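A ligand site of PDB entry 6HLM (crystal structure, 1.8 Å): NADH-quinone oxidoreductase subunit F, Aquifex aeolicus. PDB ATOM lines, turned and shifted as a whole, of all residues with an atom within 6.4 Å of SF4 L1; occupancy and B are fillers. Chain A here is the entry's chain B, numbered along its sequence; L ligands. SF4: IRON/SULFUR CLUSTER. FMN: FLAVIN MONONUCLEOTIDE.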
ATOM      1  N   ILE A 181      16.994 -25.217   9.459  1.00  0.00           N
ATOM      2  CA  ILE A 181      17.435 -23.854   9.758  1.00  0.00           C
ATOM      3  C   ILE A 181      17.271 -22.906   8.545  1.00  0.00           C
ATOM      4  O   ILE A 181      17.157 -21.690   8.747  1.00  0.00           O
ATOM      5  CB  ILE A 181      18.871 -23.832  10.338  1.00  0.00           C
ATOM      6  CG1 ILE A 181      19.190 -22.493  11.049  1.00  0.00           C
ATOM      7  CG2 ILE A 181      19.920 -24.136   9.253  1.00  0.00           C
ATOM      8  CD1 ILE A 181      18.238 -22.100  12.179  1.00  0.00           C
ATOM      9  N   HIS A 198      23.516 -20.325   7.557  1.00  0.00           N
ATOM     10  CA  HIS A 198      23.845 -19.842   8.876  1.00  0.00           C
ATOM     11  C   HIS A 198      23.072 -18.547   9.161  1.00  0.00           C
ATOM     12  O   HIS A 198      23.281 -17.559   8.464  1.00  0.00           O
ATOM     13  CB  HIS A 198      25.365 -19.623   9.040  1.00  0.00           C
ATOM     14  CG  HIS A 198      26.187 -20.886   9.064  1.00  0.00           C
ATOM     15  ND1 HIS A 198      27.542 -20.858   8.795  1.00  0.00           N
ATOM     16  CD2 HIS A 198      25.830 -22.160   9.354  1.00  0.00           C
ATOM     17  CE1 HIS A 198      27.969 -22.104   8.943  1.00  0.00           C
ATOM     18  NE2 HIS A 198      26.974 -22.920   9.272  1.00  0.00           N
ATOM     19  N   PRO A 199      22.213 -18.518  10.192  1.00  0.00           N
ATOM     20  CA  PRO A 199      21.483 -17.281  10.520  1.00  0.00           C
ATOM     21  C   PRO A 199      22.409 -16.110  10.808  1.00  0.00           C
ATOM     22  O   PRO A 199      23.534 -16.302  11.294  1.00  0.00           O
ATOM     23  CB  PRO A 199      20.685 -17.660  11.761  1.00  0.00           C
ATOM     24  CG  PRO A 199      20.434 -19.099  11.601  1.00  0.00           C
ATOM     25  CD  PRO A 199      21.756 -19.629  11.047  1.00  0.00           C
ATOM     26  N   ARG A 200      21.944 -14.894  10.477  1.00  0.00           N
ATOM     27  CA  ARG A 200      22.711 -13.668  10.751  1.00  0.00           C
ATOM     28  C   ARG A 200      22.208 -13.040  12.011  1.00  0.00           C
ATOM     29  O   ARG A 200      21.040 -13.215  12.371  1.00  0.00           O
ATOM     30  CB  ARG A 200      22.490 -12.641   9.611  1.00  0.00           C
ATOM     31  CG  ARG A 200      22.808 -13.128   8.215  1.00  0.00           C
ATOM     32  CD  ARG A 200      22.366 -12.063   7.241  1.00  0.00           C
ATOM     33  NE  ARG A 200      22.808 -12.353   5.876  1.00  0.00           N
ATOM     34  CZ  ARG A 200      22.452 -11.663   4.799  1.00  0.00           C
ATOM     35  NH1 ARG A 200      21.636 -10.623   4.911  1.00  0.00           N
ATOM     36  NH2 ARG A 200      22.903 -12.007   3.610  1.00  0.00           N
ATOM     37  N   GLU A 345      19.012 -30.436  13.738  1.00  0.00           N
ATOM     38  CA  GLU A 345      18.884 -29.175  13.006  1.00  0.00           C
ATOM     39  C   GLU A 345      19.670 -27.954  13.478  1.00  0.00           C
ATOM     40  O   GLU A 345      19.708 -26.964  12.738  1.00  0.00           O
ATOM     41  CB  GLU A 345      17.406 -28.796  12.904  1.00  0.00           C
ATOM     42  CG  GLU A 345      16.563 -29.916  12.292  1.00  0.00           C
ATOM     43  CD  GLU A 345      16.920 -30.374  10.889  1.00  0.00           C
ATOM     44  OE1 GLU A 345      17.621 -29.637  10.157  1.00  0.00           O
ATOM     45  OE2 GLU A 345      16.428 -31.442  10.487  1.00  0.00           O
ATOM     46  N   THR A 346      20.260 -27.982  14.678  1.00  0.00           N
ATOM     47  CA  THR A 346      21.079 -26.828  15.094  1.00  0.00           C
ATOM     48  C   THR A 346      22.192 -26.567  14.039  1.00  0.00           C
ATOM     49  O   THR A 346      22.799 -27.518  13.563  1.00  0.00           O
ATOM     50  CB  THR A 346      21.693 -27.046  16.491  1.00  0.00           C
ATOM     51  OG1 THR A 346      22.621 -25.989  16.711  1.00  0.00           O
ATOM     52  CG2 THR A 346      22.392 -28.414  16.655  1.00  0.00           C
ATOM     53  N   CYS A 347      22.448 -25.283  13.672  1.00  0.00           N
ATOM     54  CA  CYS A 347      23.499 -25.005  12.674  1.00  0.00           C
ATOM     55  C   CYS A 347      24.907 -25.013  13.267  1.00  0.00           C
ATOM     56  O   CYS A 347      25.885 -25.024  12.520  1.00  0.00           O
ATOM     57  CB  CYS A 347      23.224 -23.737  11.886  1.00  0.00           C
ATOM     58  SG  CYS A 347      23.680 -22.220  12.763  1.00  0.00           S
ATOM     59  N   GLY A 348      24.990 -24.978  14.596  1.00  0.00           N
ATOM     60  CA  GLY A 348      26.258 -25.060  15.324  1.00  0.00           C
ATOM     61  C   GLY A 348      27.056 -23.779  15.511  1.00  0.00           C
ATOM     62  O   GLY A 348      28.112 -23.851  16.140  1.00  0.00           O
ATOM     63  N   GLN A 349      26.588 -22.619  15.018  1.00  0.00           N
ATOM     64  CA  GLN A 349      27.300 -21.325  15.143  1.00  0.00           C
ATOM     65  C   GLN A 349      27.446 -20.871  16.594  1.00  0.00           C
ATOM     66  O   GLN A 349      28.425 -20.194  16.945  1.00  0.00           O
ATOM     67  CB  GLN A 349      26.528 -20.185  14.461  1.00  0.00           C
ATOM     68  CG  GLN A 349      26.618 -20.051  12.987  1.00  0.00           C
ATOM     69  CD  GLN A 349      26.040 -18.686  12.638  1.00  0.00           C
ATOM     70  OE1 GLN A 349      26.773 -17.679  12.589  1.00  0.00           O
ATOM     71  NE2 GLN A 349      24.717 -18.606  12.497  1.00  0.00           N
ATOM     72  N   CYS A 350      26.398 -21.171  17.410  1.00  0.00           N
ATOM     73  CA  CYS A 350      26.320 -20.737  18.806  1.00  0.00           C
ATOM     74  C   CYS A 350      26.649 -21.969  19.647  1.00  0.00           C
ATOM     75  O   CYS A 350      26.048 -23.019  19.442  1.00  0.00           O
ATOM     76  CB  CYS A 350      24.926 -20.180  19.118  1.00  0.00           C
ATOM     77  SG  CYS A 350      24.312 -18.974  17.882  1.00  0.00           S
ATOM     78  N   THR A 351      27.589 -21.835  20.589  1.00  0.00           N
ATOM     79  CA  THR A 351      28.055 -22.943  21.442  1.00  0.00           C
ATOM     80  C   THR A 351      26.936 -23.529  22.305  1.00  0.00           C
ATOM     81  O   THR A 351      26.775 -24.746  22.228  1.00  0.00           O
ATOM     82  CB  THR A 351      29.309 -22.527  22.255  1.00  0.00           C
ATOM     83  OG1 THR A 351      30.368 -22.355  21.337  1.00  0.00           O
ATOM     84  CG2 THR A 351      29.717 -23.587  23.290  1.00  0.00           C
ATOM     85  N   CYS A 353      23.732 -23.544  21.939  1.00  0.00           N
ATOM     86  CA  CYS A 353      22.791 -24.216  21.032  1.00  0.00           C
ATOM     87  C   CYS A 353      23.431 -25.495  20.466  1.00  0.00           C
ATOM     88  O   CYS A 353      22.811 -26.555  20.537  1.00  0.00           O
ATOM     89  CB  CYS A 353      22.333 -23.290  19.903  1.00  0.00           C
ATOM     90  SG  CYS A 353      21.151 -24.080  18.766  1.00  0.00           S
ATOM     91  N   ARG A 354      24.678 -25.395  19.939  1.00  0.00           N
ATOM     92  CA  ARG A 354      25.388 -26.579  19.369  1.00  0.00           C
ATOM     93  C   ARG A 354      25.503 -27.741  20.369  1.00  0.00           C
ATOM     94  O   ARG A 354      25.058 -28.860  20.078  1.00  0.00           O
ATOM     95  CB  ARG A 354      26.774 -26.167  18.824  1.00  0.00           C
ATOM     96  CG  ARG A 354      27.729 -27.308  18.433  1.00  0.00           C
ATOM     97  CD  ARG A 354      29.042 -26.804  17.819  1.00  0.00           C
ATOM     98  NE  ARG A 354      29.734 -25.817  18.644  1.00  0.00           N
ATOM     99  CZ  ARG A 354      30.648 -26.125  19.553  1.00  0.00           C
ATOM    100  NH1 ARG A 354      30.982 -27.391  19.776  1.00  0.00           N
ATOM    101  NH2 ARG A 354      31.237 -25.158  20.256  1.00  0.00           N
ATOM    102  N   CYS A 357      21.768 -28.742  22.133  1.00  0.00           N
ATOM    103  CA  CYS A 357      20.843 -29.573  21.329  1.00  0.00           C
ATOM    104  C   CYS A 357      21.343 -31.007  21.256  1.00  0.00           C
ATOM    105  O   CYS A 357      20.549 -31.952  21.352  1.00  0.00           O
ATOM    106  CB  CYS A 357      20.634 -28.983  19.945  1.00  0.00           C
ATOM    107  SG  CYS A 357      19.635 -27.465  19.918  1.00  0.00           S
ATOM    108  N   ILE A 387      20.142 -23.994  26.611  1.00  0.00           N
ATOM    109  CA  ILE A 387      20.400 -24.039  25.167  1.00  0.00           C
ATOM    110  C   ILE A 387      20.372 -22.604  24.608  1.00  0.00           C
ATOM    111  O   ILE A 387      21.133 -22.281  23.696  1.00  0.00           O
ATOM    112  CB  ILE A 387      19.385 -24.957  24.421  1.00  0.00           C
ATOM    113  CG1 ILE A 387      19.350 -26.379  25.050  1.00  0.00           C
ATOM    114  CG2 ILE A 387      19.698 -25.027  22.905  1.00  0.00           C
ATOM    115  CD1 ILE A 387      18.257 -27.407  24.449  1.00  0.00           C
ATOM    116  N   THR A 390      23.279 -16.836  24.449  1.00  0.00           N
ATOM    117  CA  THR A 390      24.105 -16.313  23.343  1.00  0.00           C
ATOM    118  C   THR A 390      23.523 -16.646  21.949  1.00  0.00           C
ATOM    119  O   THR A 390      24.105 -16.226  20.955  1.00  0.00           O
ATOM    120  CB  THR A 390      25.610 -16.748  23.460  1.00  0.00           C
ATOM    121  OG1 THR A 390      25.774 -18.053  22.896  1.00  0.00           O
ATOM    122  CG2 THR A 390      26.141 -16.712  24.919  1.00  0.00           C
ATOM    123  N   SER A 391      22.394 -17.392  21.866  1.00  0.00           N
ATOM    124  CA  SER A 391      21.777 -17.779  20.596  1.00  0.00           C
ATOM    125  C   SER A 391      21.435 -16.545  19.748  1.00  0.00           C
ATOM    126  O   SER A 391      20.988 -15.525  20.287  1.00  0.00           O
ATOM    127  CB  SER A 391      20.522 -18.609  20.835  1.00  0.00           C
ATOM    128  OG  SER A 391      19.565 -17.885  21.588  1.00  0.00           O
ATOM    129  N   ILE A 392      21.694 -16.628  18.441  1.00  0.00           N
ATOM    130  CA  ILE A 392      21.417 -15.510  17.547  1.00  0.00           C
ATOM    131  C   ILE A 392      20.141 -15.746  16.732  1.00  0.00           C
ATOM    132  O   ILE A 392      19.734 -14.847  15.998  1.00  0.00           O
ATOM    133  CB  ILE A 392      22.630 -15.082  16.692  1.00  0.00           C
ATOM    134  CG1 ILE A 392      23.134 -16.198  15.789  1.00  0.00           C
ATOM    135  CG2 ILE A 392      23.752 -14.526  17.617  1.00  0.00           C
ATOM    136  CD1 ILE A 392      24.297 -15.801  14.816  1.00  0.00           C
ATOM    137  N   CYS A 393      19.498 -16.921  16.866  1.00  0.00           N
ATOM    138  CA  CYS A 393      18.233 -17.147  16.149  1.00  0.00           C
ATOM    139  C   CYS A 393      17.233 -17.891  17.020  1.00  0.00           C
ATOM    140  O   CYS A 393      17.585 -18.359  18.115  1.00  0.00           O
ATOM    141  CB  CYS A 393      18.442 -17.822  14.783  1.00  0.00           C
ATOM    142  SG  CYS A 393      18.266 -19.618  14.804  1.00  0.00           S
ATOM    143  N   GLY A 394      15.981 -17.931  16.544  1.00  0.00           N
ATOM    144  CA  GLY A 394      14.874 -18.572  17.260  1.00  0.00           C
ATOM    145  C   GLY A 394      15.029 -20.040  17.634  1.00  0.00           C
ATOM    146  O   GLY A 394      14.424 -20.473  18.610  1.00  0.00           O
ATOM    147  N   LEU A 395      15.858 -20.819  16.881  1.00  0.00           N
ATOM    148  CA  LEU A 395      16.032 -22.257  17.197  1.00  0.00           C
ATOM    149  C   LEU A 395      16.619 -22.504  18.608  1.00  0.00           C
ATOM    150  O   LEU A 395      16.036 -23.254  19.387  1.00  0.00           O
ATOM    151  CB  LEU A 395      16.861 -22.963  16.113  1.00  0.00           C
ATOM    152  CG  LEU A 395      16.827 -24.521  16.125  1.00  0.00           C
ATOM    153  CD1 LEU A 395      17.082 -25.053  14.732  1.00  0.00           C
ATOM    154  CD2 LEU A 395      17.878 -25.102  17.076  1.00  0.00           C
ATOM    155  N   GLY A 396      17.721 -21.834  18.942  1.00  0.00           N
ATOM    156  CA  GLY A 396      18.342 -21.940  20.260  1.00  0.00           C
ATOM    157  C   GLY A 396      17.405 -21.517  21.369  1.00  0.00           C
ATOM    158  O   GLY A 396      17.385 -22.126  22.449  1.00  0.00           O
ATOM    159  N   ALA A 397      16.558 -20.493  21.074  1.00  0.00           N
ATOM    160  CA  ALA A 397      15.608 -19.957  22.054  1.00  0.00           C
ATOM    161  C   ALA A 397      14.477 -20.902  22.386  1.00  0.00           C
ATOM    162  O   ALA A 397      13.925 -20.812  23.476  1.00  0.00           O
ATOM    163  CB  ALA A 397      15.041 -18.630  21.562  1.00  0.00           C
HETATM  164 FE1  SF4 L   1      22.472 -21.859  14.656  1.00  0.00          FE
HETATM  165 FE2  SF4 L   1      21.312 -22.513  17.047  1.00  0.00          FE
HETATM  166 FE3  SF4 L   1      20.309 -20.460  15.569  1.00  0.00          FE
HETATM  167 FE4  SF4 L   1      22.740 -20.207  16.795  1.00  0.00          FE
HETATM  168  S1  SF4 L   1      20.693 -20.438  17.817  1.00  0.00           S
HETATM  169  S2  SF4 L   1      22.225 -19.551  14.697  1.00  0.00           S
HETATM  170  S3  SF4 L   1      23.550 -22.375  16.578  1.00  0.00           S
HETATM  171  S4  SF4 L   1      20.378 -22.699  15.005  1.00  0.00           S
HETATM  172  N1  FMN L   2       9.040 -19.198   8.224  1.00  0.00           N
HETATM  173  C2  FMN L   2       8.465 -19.806   7.157  1.00  0.00           C
HETATM  174  O2  FMN L   2       7.781 -19.156   6.378  1.00  0.00           O
HETATM  175  N3  FMN L   2       8.750 -21.150   6.890  1.00  0.00           N
HETATM  176  C4  FMN L   2       9.627 -21.956   7.619  1.00  0.00           C
HETATM  177  O4  FMN L   2       9.839 -23.132   7.295  1.00  0.00           O
HETATM  178  C4A FMN L   2      10.255 -21.278   8.748  1.00  0.00           C
HETATM  179  N5  FMN L   2      11.160 -21.932   9.452  1.00  0.00           N
HETATM  180  C5A FMN L   2      11.785 -21.256  10.501  1.00  0.00           C
HETATM  181  C6  FMN L   2      12.793 -21.913  11.196  1.00  0.00           C
HETATM  182  C7  FMN L   2      13.457 -21.291  12.252  1.00  0.00           C
HETATM  183  C7M FMN L   2      14.475 -22.079  13.051  1.00  0.00           C
HETATM  184  C8  FMN L   2      13.106 -19.966  12.617  1.00  0.00           C
HETATM  185  C8M FMN L   2      13.769 -19.259  13.776  1.00  0.00           C
HETATM  186  C9  FMN L   2      12.106 -19.310  11.906  1.00  0.00           C
HETATM  187  C9A FMN L   2      11.455 -19.930  10.844  1.00  0.00           C
HETATM  188  N10 FMN L   2      10.471 -19.265  10.063  1.00  0.00           N
HETATM  189  C10 FMN L   2       9.874 -19.908   8.987  1.00  0.00           C
HETATM  190  C1' FMN L   2      10.154 -17.852  10.312  1.00  0.00           C
HETATM  191  C2' FMN L   2      10.925 -16.923   9.376  1.00  0.00           C
HETATM  192  O2' FMN L   2      12.206 -16.584   9.926  1.00  0.00           O
HETATM  193  C3' FMN L   2      10.150 -15.637   9.058  1.00  0.00           C
HETATM  194  O3' FMN L   2       9.631 -15.100  10.271  1.00  0.00           O
HETATM  195  C4' FMN L   2       8.969 -15.773   8.094  1.00  0.00           C
HETATM  196  O4' FMN L   2       9.314 -16.511   6.922  1.00  0.00           O
HETATM  197  C5' FMN L   2       8.444 -14.407   7.709  1.00  0.00           C
HETATM  198  O5' FMN L   2       7.225 -14.562   6.938  1.00  0.00           O
HETATM  199  P   FMN L   2       5.811 -14.146   7.563  1.00  0.00           P
HETATM  200  O1P FMN L   2       5.914 -12.799   8.226  1.00  0.00           O
HETATM  201  O2P FMN L   2       5.441 -15.168   8.611  1.00  0.00           O
HETATM  202  O3P FMN L   2       4.868 -14.241   6.390  1.00  0.00           O
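S3 of SF4 L1 sits close to N of Gln 349. A sulfur (S2) of SF4 L1 lies close to the side-chain amide nitrogen of Gln 349 (3.5 Å). The backbone NH (N) of Cys 350 sits close to a sulfur (S3) of SF4 L1 (3.2 Å). An iron atom (FE1) of SF4 L1 is bound by the side-chain sulfur (SG) of Cys 347 (2.3 Å). The side-chain sulfur (SG) of Cys 350 binds an iron atom (FE4) of SF4 L1 (2.3 Å). The backbone NH (N) of Gly 348 sits close to a sulfur (S3) of SF4 L1, 3.6 Å away. SG of Cys 393 binds FE3 of SF4 L1 (2.3 Å). The side-chain hydroxyl (OG1) of Thr 346 lies close to a sulfur (S3) of SF4 L1 (3.7 Å). The side-chain sulfur (SG) of Cys 353 binds an iron atom (FE2) of SF4 L1 (2.3 Å). A sulfur (S4) of SF4 L1 sits close to the backbone NH (N) of Cys 347. A sulfur (S1) of SF4 L1 sits close to the backbone NH of Gly 396.
The backbone NH of Ile 392 lies close to the side-chain sulfur of Cys 350, 3.6 Å away. The side-chain sulfur of Cys 347 lies close to the backbone NH of Gln 349, at 3.7 Å. O of Cys 353 sits close to SG of Cys 357 (3.4 Å). OG1 of Thr 346 lies close to N of Gly 348 (3.3 Å). N of Cys 353 is in hydrogen-bond range of O of Ile 387, 3.4 Å away. The side-chain amide nitrogen of Gln 349 is in hydrogen-bond range of the backbone carbonyl oxygen of Pro 199 (2.9 Å). N of Leu 395 sits close to SG of Cys 393 (3.4 Å). The side-chain sulfur of Cys 353 sits close to the side-chain hydroxyl of Thr 346, at 3.2 Å.
Ile 181 touches SF4 L1. Pro 199 touches SF4 L1 (CG to S2, 3.6 Å). Ser 391 touches SF4 L1 (CB to S1, 3.5 Å). Ile 392 touches SF4 L1 (CG1 to S2, 3.6 Å). CB of Leu 395 touches S4 of SF4 L1, at 3.7 Å.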
